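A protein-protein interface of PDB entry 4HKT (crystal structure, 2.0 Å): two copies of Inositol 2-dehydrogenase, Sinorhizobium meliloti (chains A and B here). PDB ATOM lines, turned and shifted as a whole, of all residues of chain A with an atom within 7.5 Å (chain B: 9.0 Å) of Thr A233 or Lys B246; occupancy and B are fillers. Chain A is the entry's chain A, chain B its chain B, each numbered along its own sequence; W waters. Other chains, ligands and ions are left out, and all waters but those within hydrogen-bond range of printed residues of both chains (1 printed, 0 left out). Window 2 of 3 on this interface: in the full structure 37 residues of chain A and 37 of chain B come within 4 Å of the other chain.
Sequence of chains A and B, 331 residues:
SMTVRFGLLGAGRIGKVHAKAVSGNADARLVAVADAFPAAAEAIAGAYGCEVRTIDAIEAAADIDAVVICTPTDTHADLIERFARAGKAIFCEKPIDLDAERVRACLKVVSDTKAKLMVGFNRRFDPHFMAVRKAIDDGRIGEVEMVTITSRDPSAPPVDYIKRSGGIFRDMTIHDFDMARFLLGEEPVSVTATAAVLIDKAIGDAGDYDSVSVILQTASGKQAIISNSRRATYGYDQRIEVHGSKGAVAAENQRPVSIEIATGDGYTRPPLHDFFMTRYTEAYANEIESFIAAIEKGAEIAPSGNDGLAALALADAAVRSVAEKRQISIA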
ATOM      1  N   ARG A 152     -22.405   6.080  -3.510  1.00  0.00           N
ATOM      2  CA  ARG A 152     -22.897   4.738  -3.719  1.00  0.00           C
ATOM      3  C   ARG A 152     -21.869   3.964  -4.593  1.00  0.00           C
ATOM      4  O   ARG A 152     -21.489   4.418  -5.682  1.00  0.00           O
ATOM      5  CB  ARG A 152     -24.285   4.722  -4.383  1.00  0.00           C
ATOM      6  CG  ARG A 152     -25.341   5.524  -3.616  1.00  0.00           C
ATOM      7  CD  ARG A 152     -26.654   5.666  -4.364  1.00  0.00           C
ATOM      8  NE  ARG A 152     -27.617   6.280  -3.474  1.00  0.00           N
ATOM      9  CZ  ARG A 152     -28.650   7.028  -3.851  1.00  0.00           C
ATOM     10  NH1 ARG A 152     -28.932   7.240  -5.128  1.00  0.00           N
ATOM     11  NH2 ARG A 152     -29.448   7.541  -2.932  1.00  0.00           N
ATOM     12  N   ASP A 153     -21.434   2.807  -4.097  1.00  0.00           N
ATOM     13  CA  ASP A 153     -20.512   1.957  -4.817  1.00  0.00           C
ATOM     14  C   ASP A 153     -21.249   1.127  -5.870  1.00  0.00           C
ATOM     15  O   ASP A 153     -22.466   0.875  -5.772  1.00  0.00           O
ATOM     16  CB  ASP A 153     -19.795   0.999  -3.874  1.00  0.00           C
ATOM     17  CG  ASP A 153     -18.863   1.690  -2.918  1.00  0.00           C
ATOM     18  OD1 ASP A 153     -18.414   2.854  -3.156  1.00  0.00           O
ATOM     19  OD2 ASP A 153     -18.606   1.043  -1.893  1.00  0.00           O
ATOM     20  N   PRO A 154     -20.503   0.674  -6.886  1.00  0.00           N
ATOM     21  CA  PRO A 154     -21.143  -0.121  -7.917  1.00  0.00           C
ATOM     22  C   PRO A 154     -21.538  -1.510  -7.408  1.00  0.00           C
ATOM     23  O   PRO A 154     -22.506  -2.056  -7.903  1.00  0.00           O
ATOM     24  CB  PRO A 154     -20.080  -0.236  -9.030  1.00  0.00           C
ATOM     25  CG  PRO A 154     -18.896   0.485  -8.579  1.00  0.00           C
ATOM     26  CD  PRO A 154     -19.148   1.122  -7.257  1.00  0.00           C
ATOM     27  N   SER A 155     -20.799  -2.021  -6.426  1.00  0.00           N
ATOM     28  CA  SER A 155     -20.883  -3.400  -5.939  1.00  0.00           C
ATOM     29  C   SER A 155     -20.393  -3.440  -4.515  1.00  0.00           C
ATOM     30  O   SER A 155     -19.470  -2.711  -4.161  1.00  0.00           O
ATOM     31  CB  SER A 155     -19.896  -4.333  -6.667  1.00  0.00           C
ATOM     32  OG  SER A 155     -19.981  -4.247  -8.034  1.00  0.00           O
ATOM     33  N   ARG A 231     -24.155  -0.572  -2.989  1.00  0.00           N
ATOM     34  CA  ARG A 231     -24.463  -1.159  -4.315  1.00  0.00           C
ATOM     35  C   ARG A 231     -25.419  -0.291  -5.117  1.00  0.00           C
ATOM     36  O   ARG A 231     -26.565  -0.001  -4.685  1.00  0.00           O
ATOM     37  CB  ARG A 231     -25.068  -2.599  -4.203  1.00  0.00           C
ATOM     38  CG  ARG A 231     -25.396  -3.278  -5.577  1.00  0.00           C
ATOM     39  CD  ARG A 231     -26.790  -3.947  -5.653  1.00  0.00           C
ATOM     40  NE  ARG A 231     -27.608  -2.957  -5.143  1.00  0.00           N
ATOM     41  CZ  ARG A 231     -28.532  -2.991  -4.214  1.00  0.00           C
ATOM     42  NH1 ARG A 231     -29.149  -4.082  -3.748  1.00  0.00           N
ATOM     43  NH2 ARG A 231     -28.917  -1.792  -3.878  1.00  0.00           N
ATOM     44  N   ALA A 232     -24.966   0.061  -6.309  1.00  0.00           N
ATOM     45  CA  ALA A 232     -25.791   0.744  -7.301  1.00  0.00           C
ATOM     46  C   ALA A 232     -25.542   0.187  -8.712  1.00  0.00           C
ATOM     47  O   ALA A 232     -24.437   0.255  -9.216  1.00  0.00           O
ATOM     48  CB  ALA A 232     -25.540   2.248  -7.265  1.00  0.00           C
ATOM     49  N   THR A 233     -26.580  -0.320  -9.348  1.00  0.00           N
ATOM     50  CA  THR A 233     -26.444  -0.923 -10.658  1.00  0.00           C
ATOM     51  C   THR A 233     -25.980   0.091 -11.700  1.00  0.00           C
ATOM     52  O   THR A 233     -25.385  -0.303 -12.679  1.00  0.00           O
ATOM     53  CB  THR A 233     -27.773  -1.505 -11.163  1.00  0.00           C
ATOM     54  OG1 THR A 233     -28.805  -0.500 -11.145  1.00  0.00           O
ATOM     55  CG2 THR A 233     -28.191  -2.701 -10.320  1.00  0.00           C
ATOM     56  N   TYR A 234     -26.238   1.384 -11.453  1.00  0.00           N
ATOM     57  CA  TYR A 234     -25.888   2.439 -12.378  1.00  0.00           C
ATOM     58  C   TYR A 234     -24.478   2.993 -12.212  1.00  0.00           C
ATOM     59  O   TYR A 234     -24.097   3.923 -12.928  1.00  0.00           O
ATOM     60  CB  TYR A 234     -26.913   3.590 -12.296  1.00  0.00           C
ATOM     61  CG  TYR A 234     -27.251   4.039 -10.891  1.00  0.00           C
ATOM     62  CD1 TYR A 234     -26.587   5.096 -10.268  1.00  0.00           C
ATOM     63  CD2 TYR A 234     -28.260   3.414 -10.185  1.00  0.00           C
ATOM     64  CE1 TYR A 234     -26.965   5.516  -8.972  1.00  0.00           C
ATOM     65  CE2 TYR A 234     -28.612   3.824  -8.900  1.00  0.00           C
ATOM     66  CZ  TYR A 234     -27.968   4.864  -8.303  1.00  0.00           C
ATOM     67  OH  TYR A 234     -28.378   5.187  -7.003  1.00  0.00           O
ATOM     68  N   GLY A 235     -23.718   2.466 -11.263  1.00  0.00           N
ATOM     69  CA  GLY A 235     -22.316   2.834 -11.135  1.00  0.00           C
ATOM     70  C   GLY A 235     -21.946   3.647  -9.897  1.00  0.00           C
ATOM     71  O   GLY A 235     -22.633   3.668  -8.877  1.00  0.00           O
ATOM     72  N   TYR A 236     -20.801   4.279  -9.993  1.00  0.00           N
ATOM     73  CA  TYR A 236     -20.169   4.896  -8.851  1.00  0.00           C
ATOM     74  C   TYR A 236     -20.724   6.322  -8.726  1.00  0.00           C
ATOM     75  O   TYR A 236     -20.337   7.225  -9.478  1.00  0.00           O
ATOM     76  CB  TYR A 236     -18.661   4.880  -9.070  1.00  0.00           C
ATOM     77  CG  TYR A 236     -17.792   5.257  -7.903  1.00  0.00           C
ATOM     78  CD1 TYR A 236     -18.041   4.799  -6.625  1.00  0.00           C
ATOM     79  CD2 TYR A 236     -16.684   6.079  -8.093  1.00  0.00           C
ATOM     80  CE1 TYR A 236     -17.190   5.131  -5.568  1.00  0.00           C
ATOM     81  CE2 TYR A 236     -15.832   6.396  -7.043  1.00  0.00           C
ATOM     82  CZ  TYR A 236     -16.092   5.920  -5.795  1.00  0.00           C
ATOM     83  OH  TYR A 236     -15.256   6.279  -4.759  1.00  0.00           O
ATOM     84  N   PRO A 271     -24.481   4.651 -18.052  1.00  0.00           N
ATOM     85  CA  PRO A 271     -24.284   4.608 -16.605  1.00  0.00           C
ATOM     86  C   PRO A 271     -22.945   5.285 -16.240  1.00  0.00           C
ATOM     87  O   PRO A 271     -22.166   5.669 -17.139  1.00  0.00           O
ATOM     88  CB  PRO A 271     -24.286   3.098 -16.294  1.00  0.00           C
ATOM     89  CG  PRO A 271     -23.778   2.464 -17.548  1.00  0.00           C
ATOM     90  CD  PRO A 271     -24.332   3.307 -18.674  1.00  0.00           C
ATOM     91  N   LEU A 272     -22.726   5.472 -14.941  1.00  0.00           N
ATOM     92  CA  LEU A 272     -21.528   6.126 -14.420  1.00  0.00           C
ATOM     93  C   LEU A 272     -20.317   5.187 -14.517  1.00  0.00           C
ATOM     94  O   LEU A 272     -20.454   4.049 -14.953  1.00  0.00           O
ATOM     95  CB  LEU A 272     -21.732   6.542 -12.957  1.00  0.00           C
ATOM     96  CG  LEU A 272     -23.021   7.340 -12.651  1.00  0.00           C
ATOM     97  CD1 LEU A 272     -23.074   7.792 -11.196  1.00  0.00           C
ATOM     98  CD2 LEU A 272     -23.225   8.506 -13.620  1.00  0.00           C
ATOM     99  N   ASP A 274     -17.789   2.407 -13.706  1.00  0.00           N
ATOM    100  CA  ASP A 274     -18.009   1.164 -12.955  1.00  0.00           C
ATOM    101  C   ASP A 274     -16.908   0.877 -11.919  1.00  0.00           C
ATOM    102  O   ASP A 274     -17.000  -0.124 -11.219  1.00  0.00           O
ATOM    103  CB  ASP A 274     -18.177  -0.045 -13.894  1.00  0.00           C
ATOM    104  CG  ASP A 274     -16.883  -0.437 -14.602  1.00  0.00           C
ATOM    105  OD1 ASP A 274     -15.820   0.236 -14.432  1.00  0.00           O
ATOM    106  OD2 ASP A 274     -16.947  -1.432 -15.342  1.00  0.00           O
ATOM    107  N   ASP B 138     -44.166  -0.433 -10.739  1.00  0.00           N
ATOM    108  CA  ASP B 138     -43.818  -1.286 -11.858  1.00  0.00           C
ATOM    109  C   ASP B 138     -42.545  -2.126 -11.686  1.00  0.00           C
ATOM    110  O   ASP B 138     -42.213  -2.907 -12.567  1.00  0.00           O
ATOM    111  CB  ASP B 138     -43.769  -0.479 -13.146  1.00  0.00           C
ATOM    112  CG  ASP B 138     -45.129   0.014 -13.551  1.00  0.00           C
ATOM    113  OD1 ASP B 138     -46.122  -0.555 -13.081  1.00  0.00           O
ATOM    114  OD2 ASP B 138     -45.225   0.984 -14.299  1.00  0.00           O
ATOM    115  N   GLY B 139     -41.855  -2.015 -10.556  1.00  0.00           N
ATOM    116  CA  GLY B 139     -40.680  -2.853 -10.311  1.00  0.00           C
ATOM    117  C   GLY B 139     -39.399  -2.343 -10.976  1.00  0.00           C
ATOM    118  O   GLY B 139     -38.385  -3.028 -10.968  1.00  0.00           O
ATOM    119  N   ARG B 140     -39.420  -1.122 -11.492  1.00  0.00           N
ATOM    120  CA  ARG B 140     -38.304  -0.599 -12.250  1.00  0.00           C
ATOM    121  C   ARG B 140     -37.022  -0.333 -11.436  1.00  0.00           C
ATOM    122  O   ARG B 140     -35.937  -0.237 -12.018  1.00  0.00           O
ATOM    123  CB  ARG B 140     -38.760   0.623 -13.067  1.00  0.00           C
ATOM    124  CG  ARG B 140     -39.743   0.187 -14.153  1.00  0.00           C
ATOM    125  CD  ARG B 140     -40.093   1.246 -15.175  1.00  0.00           C
ATOM    126  NE  ARG B 140     -38.986   1.561 -16.081  1.00  0.00           N
ATOM    127  CZ  ARG B 140     -39.032   2.513 -17.014  1.00  0.00           C
ATOM    128  NH1 ARG B 140     -40.139   3.245 -17.183  1.00  0.00           N
ATOM    129  NH2 ARG B 140     -37.958   2.754 -17.770  1.00  0.00           N
ATOM    130  N   ILE B 141     -37.138  -0.239 -10.108  1.00  0.00           N
ATOM    131  CA  ILE B 141     -35.974  -0.064  -9.263  1.00  0.00           C
ATOM    132  C   ILE B 141     -35.827  -1.159  -8.251  1.00  0.00           C
ATOM    133  O   ILE B 141     -35.010  -1.032  -7.366  1.00  0.00           O
ATOM    134  CB  ILE B 141     -35.954   1.298  -8.515  1.00  0.00           C
ATOM    135  CG1 ILE B 141     -37.096   1.412  -7.501  1.00  0.00           C
ATOM    136  CG2 ILE B 141     -35.986   2.409  -9.520  1.00  0.00           C
ATOM    137  CD1 ILE B 141     -36.825   2.430  -6.390  1.00  0.00           C
ATOM    138  N   GLY B 142     -36.591  -2.244  -8.382  1.00  0.00           N
ATOM    139  CA  GLY B 142     -36.514  -3.349  -7.435  1.00  0.00           C
ATOM    140  C   GLY B 142     -37.070  -2.934  -6.077  1.00  0.00           C
ATOM    141  O   GLY B 142     -37.983  -2.130  -6.028  1.00  0.00           O
ATOM    142  N   GLU B 143     -36.505  -3.464  -4.993  1.00  0.00           N
ATOM    143  CA  GLU B 143     -36.990  -3.143  -3.651  1.00  0.00           C
ATOM    144  C   GLU B 143     -36.488  -1.746  -3.258  1.00  0.00           C
ATOM    145  O   GLU B 143     -35.325  -1.426  -3.467  1.00  0.00           O
ATOM    146  CB  GLU B 143     -36.517  -4.165  -2.606  1.00  0.00           C
ATOM    147  CG  GLU B 143     -37.450  -5.340  -2.342  1.00  0.00           C
ATOM    148  CD  GLU B 143     -38.782  -4.912  -1.748  1.00  0.00           C
ATOM    149  OE1 GLU B 143     -38.830  -4.417  -0.573  1.00  0.00           O
ATOM    150  OE2 GLU B 143     -39.776  -5.048  -2.491  1.00  0.00           O
ATOM    151  N   VAL B 144     -37.355  -0.936  -2.680  1.00  0.00           N
ATOM    152  CA  VAL B 144     -36.953   0.407  -2.213  1.00  0.00           C
ATOM    153  C   VAL B 144     -35.923   0.220  -1.111  1.00  0.00           C
ATOM    154  O   VAL B 144     -36.072  -0.668  -0.291  1.00  0.00           O
ATOM    155  CB  VAL B 144     -38.161   1.189  -1.697  1.00  0.00           C
ATOM    156  CG1 VAL B 144     -37.745   2.456  -0.947  1.00  0.00           C
ATOM    157  CG2 VAL B 144     -39.047   1.551  -2.857  1.00  0.00           C
ATOM    158  N   GLU B 145     -34.846   1.002  -1.140  1.00  0.00           N
ATOM    159  CA  GLU B 145     -33.848   0.986  -0.064  1.00  0.00           C
ATOM    160  C   GLU B 145     -33.689   2.381   0.658  1.00  0.00           C
ATOM    161  O   GLU B 145     -33.783   2.481   1.874  1.00  0.00           O
ATOM    162  CB  GLU B 145     -32.513   0.518  -0.648  1.00  0.00           C
ATOM    163  CG  GLU B 145     -32.563  -0.973  -0.999  1.00  0.00           C
ATOM    164  CD  GLU B 145     -31.356  -1.535  -1.734  1.00  0.00           C
ATOM    165  OE1 GLU B 145     -30.328  -0.837  -2.048  1.00  0.00           O
ATOM    166  OE2 GLU B 145     -31.498  -2.756  -2.044  1.00  0.00           O
ATOM    167  N   VAL B 242     -35.265   8.019  -5.139  1.00  0.00           N
ATOM    168  CA  VAL B 242     -35.444   6.732  -4.514  1.00  0.00           C
ATOM    169  C   VAL B 242     -34.432   5.724  -5.092  1.00  0.00           C
ATOM    170  O   VAL B 242     -34.436   5.432  -6.312  1.00  0.00           O
ATOM    171  CB  VAL B 242     -36.865   6.190  -4.700  1.00  0.00           C
ATOM    172  CG1 VAL B 242     -37.010   4.886  -3.932  1.00  0.00           C
ATOM    173  CG2 VAL B 242     -37.900   7.200  -4.245  1.00  0.00           C
ATOM    174  N   HIS B 243     -33.549   5.264  -4.224  1.00  0.00           N
ATOM    175  CA  HIS B 243     -32.552   4.273  -4.581  1.00  0.00           C
ATOM    176  C   HIS B 243     -33.131   2.934  -4.170  1.00  0.00           C
ATOM    177  O   HIS B 243     -33.622   2.805  -3.065  1.00  0.00           O
ATOM    178  CB  HIS B 243     -31.249   4.545  -3.865  1.00  0.00           C
ATOM    179  CG  HIS B 243     -30.188   3.514  -4.104  1.00  0.00           C
ATOM    180  ND1 HIS B 243     -29.623   3.297  -5.341  1.00  0.00           N
ATOM    181  CD2 HIS B 243     -29.577   2.654  -3.256  1.00  0.00           C
ATOM    182  CE1 HIS B 243     -28.728   2.339  -5.250  1.00  0.00           C
ATOM    183  NE2 HIS B 243     -28.661   1.948  -3.991  1.00  0.00           N
ATOM    184  N   GLY B 244     -33.091   1.976  -5.096  1.00  0.00           N
ATOM    185  CA  GLY B 244     -33.598   0.611  -4.892  1.00  0.00           C
ATOM    186  C   GLY B 244     -32.590  -0.433  -5.331  1.00  0.00           C
ATOM    187  O   GLY B 244     -31.481  -0.083  -5.796  1.00  0.00           O
ATOM    188  N   SER B 245     -32.950  -1.715  -5.182  1.00  0.00           N
ATOM    189  CA  SER B 245     -31.997  -2.820  -5.414  1.00  0.00           C
ATOM    190  C   SER B 245     -31.556  -2.901  -6.874  1.00  0.00           C
ATOM    191  O   SER B 245     -30.411  -3.270  -7.182  1.00  0.00           O
ATOM    192  CB  SER B 245     -32.590  -4.184  -4.930  1.00  0.00           C
ATOM    193  OG  SER B 245     -33.859  -4.434  -5.517  1.00  0.00           O
ATOM    194  N   LYS B 246     -32.445  -2.506  -7.784  1.00  0.00           N
ATOM    195  CA  LYS B 246     -32.196  -2.634  -9.212  1.00  0.00           C
ATOM    196  C   LYS B 246     -31.880  -1.330  -9.938  1.00  0.00           C
ATOM    197  O   LYS B 246     -31.515  -1.326 -11.135  1.00  0.00           O
ATOM    198  CB  LYS B 246     -33.419  -3.253  -9.878  1.00  0.00           C
ATOM    199  CG  LYS B 246     -33.598  -4.745  -9.608  1.00  0.00           C
ATOM    200  CD  LYS B 246     -34.836  -5.187 -10.414  1.00  0.00           C
ATOM    201  CE  LYS B 246     -35.045  -6.680 -10.402  1.00  0.00           C
ATOM    202  NZ  LYS B 246     -35.154  -7.173  -9.022  1.00  0.00           N
ATOM    203  N   GLY B 247     -32.077  -0.207  -9.252  1.00  0.00           N
ATOM    204  CA  GLY B 247     -31.724   1.062  -9.814  1.00  0.00           C
ATOM    205  C   GLY B 247     -32.209   2.222  -8.969  1.00  0.00           C
ATOM    206  O   GLY B 247     -32.567   2.016  -7.829  1.00  0.00           O
ATOM    207  N   ALA B 248     -32.253   3.415  -9.543  1.00  0.00           N
ATOM    208  CA  ALA B 248     -32.745   4.583  -8.842  1.00  0.00           C
ATOM    209  C   ALA B 248     -33.692   5.343  -9.744  1.00  0.00           C
ATOM    210  O   ALA B 248     -33.607   5.253 -10.967  1.00  0.00           O
ATOM    211  CB  ALA B 248     -31.600   5.499  -8.358  1.00  0.00           C
ATOM    212  N   VAL B 249     -34.595   6.090  -9.123  1.00  0.00           N
ATOM    213  CA  VAL B 249     -35.531   6.941  -9.830  1.00  0.00           C
ATOM    214  C   VAL B 249     -35.642   8.283  -9.096  1.00  0.00           C
ATOM    215  O   VAL B 249     -35.652   8.333  -7.849  1.00  0.00           O
ATOM    216  CB  VAL B 249     -36.903   6.277 -10.003  1.00  0.00           C
ATOM    217  CG1 VAL B 249     -37.512   5.875  -8.681  1.00  0.00           C
ATOM    218  CG2 VAL B 249     -37.848   7.181 -10.796  1.00  0.00           C
HETATM  219  O   HOH W   1     -29.108  -0.619  -7.429  1.00  0.00           O
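NH2 of Arg A231 is in salt-bridge range of OE1 of Glu B145, at 2.5 Å. The backbone carbonyl oxygen (O) of Arg A231 lies within hydrogen-bond range of a ring nitrogen (NE2) of His B243 (2.9 Å). NE of Arg A231 is in hydrogen-bond range of O of Ser B245, 3.5 Å away. The backbone carbonyl oxygen (O) of Lys B246 is in hydrogen-bond range of the side-chain hydroxyl (OG1) of Thr A233 (2.8 Å). ND1 of His B243 is in hydrogen-bond range of OH of Tyr A234, 2.8 Å away.
The side-chain hydroxyl (OH) of Tyr A234 sits at hydrogen-bond distance from the guanidinium group (NH1) of Arg A152. The backbone carbonyl oxygen of Asp A153 lies within hydrogen-bond range of the backbone NH of Ala A232 (2.7 Å). N of Leu A272 sits at hydrogen-bond distance from O of Tyr A234 (2.9 Å). The backbone NH (N) of Lys B246 sits at hydrogen-bond distance from the backbone carbonyl oxygen (O) of Ile B141, 3.0 Å away. N of Glu B143 lies within hydrogen-bond range of OG of Ser B245 (2.9 Å). The backbone carbonyl oxygen of His B243 sits at hydrogen-bond distance from the backbone NH of Glu B145 (2.9 Å).
Among the printed residues, merely in contact across the chains: Arg A152 with His B243, Arg A231 with Gly B244, Ala A232 with His B243, Thr A233 with Ser B245, Thr A233 with Gly B247, Tyr A234 with Gly B247 and Tyr A234 with Ala B248.
Of the printed residues of chain B, Thr A233 touches Ser B245, Lys B246 and Gly B247. Of chain A, only Thr A233 (2.8 Å) comes within 4 Å of Lys B246. Ser B245 touches two residues of chain A. Of the printed residues of chain A, Gly B247 touches Thr A233 (3.6 Å) and Tyr A234 (3.9 Å). Of the printed residues of chain A, Glu B145 touches Arg A231. Gly B142 touches none of the printed residues of chain A. Asp B138 touches none of the printed residues of chain A. The nearest residue of chain B that does not touch Thr A233 is His B243 (5.3 Å). The nearest residue of chain A that does not touch Lys B246 is Arg A231 (5.3 Å).
Of the 16 printed residues of chain B, 7 touch a printed residue of chain A. Printed residues of chain B that touch a printed residue of chain A: Glu B145, His B243, Gly B244, Ser B245, Lys B246, Gly B247 and Ala B248. Hydrophobic or aromatic side chains of chain B that line the printed part of chain A: His B243 and Ala B248. Of the 13 printed residues of chain A, 5 touch a printed residue of chain B. Printed residues of chain A that touch a printed residue of chain B: Arg A152, Arg A231, Ala A232, Thr A233 and Tyr A234. Among the printed residues, 12 pairs touch across the chains. Among the printed residues, Asp or Glu carboxylates within 4 Å of a Lys or Arg side-chain nitrogen of the other chain: Arg A231 with Glu B145.
No position is printed for both chains.
Water W1 lies within hydrogen-bond range of O of Gly B244 (2.9 Å), O of Ser B245 (3.0 Å) and N of Thr A233 (3.2 Å).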
